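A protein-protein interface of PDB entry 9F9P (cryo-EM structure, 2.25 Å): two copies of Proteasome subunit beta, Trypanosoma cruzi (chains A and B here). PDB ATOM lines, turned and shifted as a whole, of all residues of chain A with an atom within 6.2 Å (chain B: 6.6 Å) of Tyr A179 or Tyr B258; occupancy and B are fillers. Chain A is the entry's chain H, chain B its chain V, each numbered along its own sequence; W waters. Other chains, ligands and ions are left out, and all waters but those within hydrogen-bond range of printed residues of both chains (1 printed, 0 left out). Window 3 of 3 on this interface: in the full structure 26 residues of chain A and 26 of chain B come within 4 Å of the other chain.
OD1 of Asp A194 lies within hydrogen-bond range of OH of Tyr B258. The side-chain carboxylate (OD1) of Asp A194 is in salt-bridge range of the guanidinium group (NH2) of Arg B220 (2.7 Å). OH of Tyr B258 is in hydrogen-bond range of OH of Tyr A179, 2.8 Å away. O of Tyr A197 sits at hydrogen-bond distance from NZ of Lys B257. O of Asp A194 lies within hydrogen-bond range of NZ of Lys B257, 2.9 Å away. O of Phe A193 lies within hydrogen-bond range of NZ of Lys B257.
The guanidinium group (NE) of Arg B220 lies close to the side-chain sulfur (SD) of Met B252, 3.5 Å away. NH2 of Arg B220 is in hydrogen-bond range of OH of Tyr B258 (3.2 Å). The side-chain carboxylate of Asp B255 lies within salt-bridge range of the side-chain amino group of Lys B257, at 3.1 Å. The side-chain hydroxyl (OH) of Tyr A197 sits at hydrogen-bond distance from the side-chain carboxylate (OD2) of Asp A178. The side-chain hydroxyl of Tyr A197 sits at hydrogen-bond distance from the backbone carbonyl oxygen of Ala A61. The side-chain hydroxyl of Tyr B250 is in hydrogen-bond range of the side-chain carboxylate of Asp B255 (2.8 Å).
Among the printed residues, merely in contact across the chains: Tyr A179 with Arg B220, Tyr A190 with Arg B220, Asp A194 with Tyr B250 and Asp A194 with Asp B255.
Tyr A179 touches just these residues of chain B: Arg B220 (3.5 Å) and Tyr B258 (2.8 Å). Printed residues of chain A within 4 Å of Tyr B250: Asp A194 (3.4 Å). Printed residues of chain A within 4 Å of Lys B257: Phe A193 (3.4 Å), Asp A194 (2.9 Å) and Tyr A197 (3.5 Å). Tyr B258 touches just these residues of chain A: Tyr A179 (2.8 Å) and Asp A194 (2.5 Å). Arg B259 touches none of the printed residues of chain A. The nearest printed residue of chain A that does not touch Arg B220 is Phe A193 (6.0 Å).
Of the 12 printed residues of chain B, 5 touch a printed residue of chain A. Hydrophobic or aromatic side chains of chain B that line the printed part of chain A: Tyr B250 and Tyr B258. Of the 13 printed residues of chain A, 5 touch a printed residue of chain B. Hydrophobic or aromatic side chains of chain A within 4 Å of the printed part of chain B: Tyr A179, Tyr A190 and Tyr A197.
No position is printed for both chains.
Water W1 bridges the side-chain hydroxyl of Tyr A179 (3.2 Å) and the guanidinium group of Arg B220 (3.2 Å).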
ATOM      1  N   ALA A  59      -9.211   0.740   4.795  1.00  0.00           N
ATOM      2  CA  ALA A  59      -9.052   2.174   4.714  1.00  0.00           C
ATOM      3  C   ALA A  59      -7.582   2.500   4.612  1.00  0.00           C
ATOM      4  O   ALA A  59      -6.791   1.925   5.300  1.00  0.00           O
ATOM      5  CB  ALA A  59      -9.672   2.857   5.901  1.00  0.00           C
ATOM      6  N   VAL A  60      -7.267   3.483   3.818  1.00  0.00           N
ATOM      7  CA  VAL A  60      -5.907   3.874   3.543  1.00  0.00           C
ATOM      8  C   VAL A  60      -5.760   5.377   3.630  1.00  0.00           C
ATOM      9  O   VAL A  60      -6.529   6.105   3.039  1.00  0.00           O
ATOM     10  CB  VAL A  60      -5.593   3.424   2.106  1.00  0.00           C
ATOM     11  CG1 VAL A  60      -4.201   3.798   1.713  1.00  0.00           C
ATOM     12  CG2 VAL A  60      -5.791   1.928   1.947  1.00  0.00           C
ATOM     13  N   ALA A  61      -4.696   5.851   4.211  1.00  0.00           N
ATOM     14  CA  ALA A  61      -4.463   7.291   4.265  1.00  0.00           C
ATOM     15  C   ALA A  61      -3.743   7.750   2.991  1.00  0.00           C
ATOM     16  O   ALA A  61      -3.003   6.979   2.390  1.00  0.00           O
ATOM     17  CB  ALA A  61      -3.663   7.605   5.497  1.00  0.00           C
ATOM     18  N   VAL A 165      -6.853   7.117  10.281  1.00  0.00           N
ATOM     19  CA  VAL A 165      -7.395   5.753  10.231  1.00  0.00           C
ATOM     20  C   VAL A 165      -7.183   5.072  11.571  1.00  0.00           C
ATOM     21  O   VAL A 165      -6.079   5.036  12.049  1.00  0.00           O
ATOM     22  CB  VAL A 165      -6.703   4.929   9.111  1.00  0.00           C
ATOM     23  CG1 VAL A 165      -7.143   3.484   9.067  1.00  0.00           C
ATOM     24  CG2 VAL A 165      -6.895   5.523   7.743  1.00  0.00           C
ATOM     25  N   LEU A 177      -3.207   3.954  12.608  1.00  0.00           N
ATOM     26  CA  LEU A 177      -2.349   3.414  11.558  1.00  0.00           C
ATOM     27  C   LEU A 177      -2.420   4.249  10.298  1.00  0.00           C
ATOM     28  O   LEU A 177      -3.297   5.071  10.167  1.00  0.00           O
ATOM     29  CB  LEU A 177      -2.882   2.036  11.170  1.00  0.00           C
ATOM     30  CG  LEU A 177      -2.941   1.007  12.286  1.00  0.00           C
ATOM     31  CD1 LEU A 177      -3.989  -0.050  11.993  1.00  0.00           C
ATOM     32  CD2 LEU A 177      -1.575   0.384  12.501  1.00  0.00           C
ATOM     33  N   ASP A 178      -1.630   3.843   9.322  1.00  0.00           N
ATOM     34  CA  ASP A 178      -1.602   4.377   7.970  1.00  0.00           C
ATOM     35  C   ASP A 178      -2.557   3.641   7.028  1.00  0.00           C
ATOM     36  O   ASP A 178      -3.076   4.213   6.095  1.00  0.00           O
ATOM     37  CB  ASP A 178      -0.187   4.202   7.427  1.00  0.00           C
ATOM     38  CG  ASP A 178       0.288   5.489   6.805  1.00  0.00           C
ATOM     39  OD1 ASP A 178       0.628   6.433   7.592  1.00  0.00           O
ATOM     40  OD2 ASP A 178       0.236   5.575   5.538  1.00  0.00           O
ATOM     41  N   TYR A 179      -2.789   2.351   7.284  1.00  0.00           N
ATOM     42  CA  TYR A 179      -3.832   1.622   6.602  1.00  0.00           C
ATOM     43  C   TYR A 179      -4.370   0.548   7.522  1.00  0.00           C
ATOM     44  O   TYR A 179      -3.680   0.138   8.413  1.00  0.00           O
ATOM     45  CB  TYR A 179      -3.287   1.067   5.293  1.00  0.00           C
ATOM     46  CG  TYR A 179      -2.301  -0.067   5.385  1.00  0.00           C
ATOM     47  CD1 TYR A 179      -2.726  -1.352   5.658  1.00  0.00           C
ATOM     48  CD2 TYR A 179      -0.941   0.133   5.244  1.00  0.00           C
ATOM     49  CE1 TYR A 179      -1.825  -2.405   5.808  1.00  0.00           C
ATOM     50  CE2 TYR A 179      -0.025  -0.912   5.375  1.00  0.00           C
ATOM     51  CZ  TYR A 179      -0.468  -2.198   5.627  1.00  0.00           C
ATOM     52  OH  TYR A 179       0.360  -3.301   5.740  1.00  0.00           O
ATOM     53  N   ALA A 180      -5.588   0.085   7.275  1.00  0.00           N
ATOM     54  CA  ALA A 180      -6.163  -0.987   8.048  1.00  0.00           C
ATOM     55  C   ALA A 180      -6.919  -1.956   7.145  1.00  0.00           C
ATOM     56  O   ALA A 180      -7.522  -1.507   6.180  1.00  0.00           O
ATOM     57  CB  ALA A 180      -7.092  -0.356   9.053  1.00  0.00           C
ATOM     58  N   LEU A 181      -6.907  -3.256   7.478  1.00  0.00           N
ATOM     59  CA  LEU A 181      -7.652  -4.277   6.739  1.00  0.00           C
ATOM     60  C   LEU A 181      -8.581  -5.032   7.688  1.00  0.00           C
ATOM     61  O   LEU A 181      -8.261  -5.230   8.824  1.00  0.00           O
ATOM     62  CB  LEU A 181      -6.667  -5.258   6.099  1.00  0.00           C
ATOM     63  CG  LEU A 181      -5.521  -4.589   5.355  1.00  0.00           C
ATOM     64  CD1 LEU A 181      -4.436  -5.573   4.948  1.00  0.00           C
ATOM     65  CD2 LEU A 181      -6.060  -3.903   4.118  1.00  0.00           C
ATOM     66  N   TYR A 190      -2.666  -8.888   3.160  1.00  0.00           N
ATOM     67  CA  TYR A 190      -1.426  -8.534   3.851  1.00  0.00           C
ATOM     68  C   TYR A 190      -0.245  -8.530   2.893  1.00  0.00           C
ATOM     69  O   TYR A 190       0.458  -7.530   2.830  1.00  0.00           O
ATOM     70  CB  TYR A 190      -1.170  -9.385   5.092  1.00  0.00           C
ATOM     71  CG  TYR A 190      -2.091  -8.984   6.211  1.00  0.00           C
ATOM     72  CD1 TYR A 190      -1.980  -7.724   6.764  1.00  0.00           C
ATOM     73  CD2 TYR A 190      -3.162  -9.794   6.612  1.00  0.00           C
ATOM     74  CE1 TYR A 190      -2.857  -7.301   7.749  1.00  0.00           C
ATOM     75  CE2 TYR A 190      -4.066  -9.373   7.588  1.00  0.00           C
ATOM     76  CZ  TYR A 190      -3.913  -8.109   8.150  1.00  0.00           C
ATOM     77  OH  TYR A 190      -4.761  -7.610   9.133  1.00  0.00           O
ATOM     78  N   PHE A 193      -0.296  -5.606   0.057  1.00  0.00           N
ATOM     79  CA  PHE A 193       0.155  -4.330   0.592  1.00  0.00           C
ATOM     80  C   PHE A 193       1.640  -4.323   0.933  1.00  0.00           C
ATOM     81  O   PHE A 193       2.311  -3.340   0.707  1.00  0.00           O
ATOM     82  CB  PHE A 193      -0.586  -3.999   1.892  1.00  0.00           C
ATOM     83  CG  PHE A 193      -1.883  -3.272   1.703  1.00  0.00           C
ATOM     84  CD1 PHE A 193      -2.970  -3.909   1.131  1.00  0.00           C
ATOM     85  CD2 PHE A 193      -1.995  -1.934   2.040  1.00  0.00           C
ATOM     86  CE1 PHE A 193      -4.177  -3.245   0.943  1.00  0.00           C
ATOM     87  CE2 PHE A 193      -3.176  -1.252   1.782  1.00  0.00           C
ATOM     88  CZ  PHE A 193      -4.279  -1.910   1.251  1.00  0.00           C
ATOM     89  N   ASP A 194       2.153  -5.388   1.546  1.00  0.00           N
ATOM     90  CA  ASP A 194       3.580  -5.492   1.829  1.00  0.00           C
ATOM     91  C   ASP A 194       4.415  -5.312   0.567  1.00  0.00           C
ATOM     92  O   ASP A 194       5.417  -4.617   0.601  1.00  0.00           O
ATOM     93  CB  ASP A 194       3.930  -6.813   2.534  1.00  0.00           C
ATOM     94  CG  ASP A 194       3.577  -6.923   4.016  1.00  0.00           C
ATOM     95  OD1 ASP A 194       3.177  -5.917   4.627  1.00  0.00           O
ATOM     96  OD2 ASP A 194       3.693  -8.040   4.563  1.00  0.00           O
ATOM     97  N   TYR A 197       2.223  -1.260  -1.646  1.00  0.00           N
ATOM     98  CA  TYR A 197       1.729  -0.019  -1.053  1.00  0.00           C
ATOM     99  C   TYR A 197       2.861   0.936  -0.700  1.00  0.00           C
ATOM    100  O   TYR A 197       3.832   0.530  -0.096  1.00  0.00           O
ATOM    101  CB  TYR A 197       0.962  -0.264   0.265  1.00  0.00           C
ATOM    102  CG  TYR A 197       0.562   0.988   1.035  1.00  0.00           C
ATOM    103  CD1 TYR A 197      -0.480   1.793   0.597  1.00  0.00           C
ATOM    104  CD2 TYR A 197       1.239   1.415   2.178  1.00  0.00           C
ATOM    105  CE1 TYR A 197      -0.871   2.935   1.285  1.00  0.00           C
ATOM    106  CE2 TYR A 197       0.868   2.565   2.882  1.00  0.00           C
ATOM    107  CZ  TYR A 197      -0.200   3.339   2.432  1.00  0.00           C
ATOM    108  OH  TYR A 197      -0.628   4.525   3.070  1.00  0.00           O
ATOM    109  N   ARG B 220       4.658 -12.847   7.419  1.00  0.00           N
ATOM    110  CA  ARG B 220       3.346 -12.676   8.018  1.00  0.00           C
ATOM    111  C   ARG B 220       2.870 -13.875   8.827  1.00  0.00           C
ATOM    112  O   ARG B 220       1.940 -13.694   9.589  1.00  0.00           O
ATOM    113  CB  ARG B 220       2.322 -12.343   6.918  1.00  0.00           C
ATOM    114  CG  ARG B 220       2.483 -10.942   6.334  1.00  0.00           C
ATOM    115  CD  ARG B 220       2.068  -9.898   7.361  1.00  0.00           C
ATOM    116  NE  ARG B 220       2.161  -8.547   6.865  1.00  0.00           N
ATOM    117  CZ  ARG B 220       1.689  -7.467   7.485  1.00  0.00           C
ATOM    118  NH1 ARG B 220       1.084  -7.544   8.660  1.00  0.00           N
ATOM    119  NH2 ARG B 220       1.859  -6.297   6.912  1.00  0.00           N
ATOM    120  N   TYR B 250      12.971 -10.187   1.439  1.00  0.00           N
ATOM    121  CA  TYR B 250      11.977  -9.315   2.053  1.00  0.00           C
ATOM    122  C   TYR B 250      11.802  -9.666   3.529  1.00  0.00           C
ATOM    123  O   TYR B 250      11.687 -10.848   3.882  1.00  0.00           O
ATOM    124  CB  TYR B 250      10.593  -9.458   1.402  1.00  0.00           C
ATOM    125  CG  TYR B 250       9.553  -8.558   2.008  1.00  0.00           C
ATOM    126  CD1 TYR B 250       9.503  -7.215   1.669  1.00  0.00           C
ATOM    127  CD2 TYR B 250       8.730  -8.999   3.048  1.00  0.00           C
ATOM    128  CE1 TYR B 250       8.605  -6.346   2.286  1.00  0.00           C
ATOM    129  CE2 TYR B 250       7.859  -8.130   3.707  1.00  0.00           C
ATOM    130  CZ  TYR B 250       7.793  -6.796   3.324  1.00  0.00           C
ATOM    131  OH  TYR B 250       6.916  -5.921   3.952  1.00  0.00           O
ATOM    132  N   CYS B 251      11.703  -8.637   4.388  1.00  0.00           N
ATOM    133  CA  CYS B 251      11.128  -8.814   5.730  1.00  0.00           C
ATOM    134  C   CYS B 251      10.506  -7.499   6.213  1.00  0.00           C
ATOM    135  O   CYS B 251      10.932  -6.436   5.776  1.00  0.00           O
ATOM    136  CB  CYS B 251      12.206  -9.285   6.722  1.00  0.00           C
ATOM    137  SG  CYS B 251      13.617  -8.145   6.741  1.00  0.00           S
ATOM    138  N   MET B 252       9.588  -7.560   7.179  1.00  0.00           N
ATOM    139  CA  MET B 252       8.941  -6.342   7.664  1.00  0.00           C
ATOM    140  C   MET B 252       9.934  -5.437   8.395  1.00  0.00           C
ATOM    141  O   MET B 252       9.863  -4.223   8.222  1.00  0.00           O
ATOM    142  CB  MET B 252       7.728  -6.651   8.550  1.00  0.00           C
ATOM    143  CG  MET B 252       6.560  -7.163   7.716  1.00  0.00           C
ATOM    144  SD  MET B 252       4.991  -7.422   8.562  1.00  0.00           S
ATOM    145  CE  MET B 252       5.496  -8.417   9.968  1.00  0.00           C
ATOM    146  N   GLU B 253      10.877  -6.046   9.130  1.00  0.00           N
ATOM    147  CA  GLU B 253      11.843  -5.368   9.985  1.00  0.00           C
ATOM    148  C   GLU B 253      12.720  -4.396   9.207  1.00  0.00           C
ATOM    149  O   GLU B 253      13.286  -3.504   9.823  1.00  0.00           O
ATOM    150  CB  GLU B 253      12.825  -6.338  10.658  1.00  0.00           C
ATOM    151  CG  GLU B 253      12.249  -7.371  11.653  1.00  0.00           C
ATOM    152  CD  GLU B 253      11.759  -8.722  11.107  1.00  0.00           C
ATOM    153  OE1 GLU B 253      11.235  -8.722   9.953  1.00  0.00           O
ATOM    154  OE2 GLU B 253      11.820  -9.765  11.841  1.00  0.00           O
ATOM    155  N   ASP B 255      11.699  -3.100   5.932  1.00  0.00           N
ATOM    156  CA  ASP B 255      10.836  -2.345   5.038  1.00  0.00           C
ATOM    157  C   ASP B 255      10.680  -0.921   5.584  1.00  0.00           C
ATOM    158  O   ASP B 255      10.265  -0.751   6.734  1.00  0.00           O
ATOM    159  CB  ASP B 255       9.480  -3.049   4.938  1.00  0.00           C
ATOM    160  CG  ASP B 255       8.538  -2.513   3.871  1.00  0.00           C
ATOM    161  OD1 ASP B 255       8.877  -1.474   3.229  1.00  0.00           O
ATOM    162  OD2 ASP B 255       7.486  -3.169   3.655  1.00  0.00           O
ATOM    163  N   PRO B 256      11.020   0.144   4.822  1.00  0.00           N
ATOM    164  CA  PRO B 256      10.960   1.515   5.344  1.00  0.00           C
ATOM    165  C   PRO B 256       9.571   2.054   5.698  1.00  0.00           C
ATOM    166  O   PRO B 256       9.482   2.961   6.517  1.00  0.00           O
ATOM    167  CB  PRO B 256      11.569   2.365   4.210  1.00  0.00           C
ATOM    168  CG  PRO B 256      12.351   1.363   3.365  1.00  0.00           C
ATOM    169  CD  PRO B 256      11.519   0.098   3.433  1.00  0.00           C
ATOM    170  N   LYS B 257       8.494   1.482   5.151  1.00  0.00           N
ATOM    171  CA  LYS B 257       7.159   1.910   5.533  1.00  0.00           C
ATOM    172  C   LYS B 257       6.731   1.417   6.924  1.00  0.00           C
ATOM    173  O   LYS B 257       5.667   1.813   7.396  1.00  0.00           O
ATOM    174  CB  LYS B 257       6.108   1.511   4.491  1.00  0.00           C
ATOM    175  CG  LYS B 257       5.793   0.027   4.335  1.00  0.00           C
ATOM    176  CD  LYS B 257       4.596  -0.204   3.392  1.00  0.00           C
ATOM    177  CE  LYS B 257       4.374  -1.642   2.946  1.00  0.00           C
ATOM    178  NZ  LYS B 257       5.269  -2.018   1.819  1.00  0.00           N
ATOM    179  N   TYR B 258       7.540   0.589   7.594  1.00  0.00           N
ATOM    180  CA  TYR B 258       7.231   0.121   8.936  1.00  0.00           C
ATOM    181  C   TYR B 258       8.329   0.535   9.914  1.00  0.00           C
ATOM    182  O   TYR B 258       8.417  -0.020  10.999  1.00  0.00           O
ATOM    183  CB  TYR B 258       7.100  -1.409   8.998  1.00  0.00           C
ATOM    184  CG  TYR B 258       6.027  -2.011   8.130  1.00  0.00           C
ATOM    185  CD1 TYR B 258       4.695  -1.614   8.250  1.00  0.00           C
ATOM    186  CD2 TYR B 258       6.342  -2.969   7.179  1.00  0.00           C
ATOM    187  CE1 TYR B 258       3.700  -2.180   7.461  1.00  0.00           C
ATOM    188  CE2 TYR B 258       5.370  -3.519   6.358  1.00  0.00           C
ATOM    189  CZ  TYR B 258       4.045  -3.118   6.493  1.00  0.00           C
ATOM    190  OH  TYR B 258       3.089  -3.642   5.661  1.00  0.00           O
ATOM    191  N   ARG B 259       9.165   1.502   9.548  1.00  0.00           N
ATOM    192  CA  ARG B 259      10.222   1.941  10.442  1.00  0.00           C
ATOM    193  C   ARG B 259       9.653   2.799  11.584  1.00  0.00           C
ATOM    194  O   ARG B 259       9.943   2.540  12.748  1.00  0.00           O
ATOM    195  CB  ARG B 259      11.285   2.692   9.641  1.00  0.00           C
ATOM    196  CG  ARG B 259      12.618   2.801  10.369  1.00  0.00           C
ATOM    197  CD  ARG B 259      13.684   3.536   9.564  1.00  0.00           C
ATOM    198  NE  ARG B 259      13.181   4.767   8.951  1.00  0.00           N
ATOM    199  CZ  ARG B 259      12.681   5.811   9.615  1.00  0.00           C
ATOM    200  NH1 ARG B 259      12.698   5.840  10.937  1.00  0.00           N
ATOM    201  NH2 ARG B 259      12.171   6.835   8.949  1.00  0.00           N
ATOM    202  N   ASP B 260       8.857   3.821  11.261  1.00  0.00           N
ATOM    203  CA  ASP B 260       8.308   4.731  12.258  1.00  0.00           C
ATOM    204  C   ASP B 260       7.163   4.072  13.054  1.00  0.00           C
ATOM    205  O   ASP B 260       6.224   3.497  12.497  1.00  0.00           O
ATOM    206  CB  ASP B 260       7.855   6.048  11.607  1.00  0.00           C
ATOM    207  CG  ASP B 260       6.575   5.925  10.775  1.00  0.00           C
ATOM    208  OD1 ASP B 260       6.633   5.321   9.665  1.00  0.00           O
ATOM    209  OD2 ASP B 260       5.509   6.394  11.252  1.00  0.00           O
ATOM    210  N   LEU B 261       7.211   4.203  14.383  1.00  0.00           N
ATOM    211  CA  LEU B 261       6.232   3.552  15.227  1.00  0.00           C
ATOM    212  C   LEU B 261       4.915   4.305  15.219  1.00  0.00           C
ATOM    213  O   LEU B 261       4.892   5.513  15.184  1.00  0.00           O
ATOM    214  CB  LEU B 261       6.786   3.468  16.646  1.00  0.00           C
ATOM    215  CG  LEU B 261       8.061   2.641  16.812  1.00  0.00           C
ATOM    216  CD1 LEU B 261       8.621   2.780  18.205  1.00  0.00           C
ATOM    217  CD2 LEU B 261       7.809   1.164  16.534  1.00  0.00           C
HETATM  218  O   HOH W   1       0.364  -4.156   8.830  1.00  0.00           O
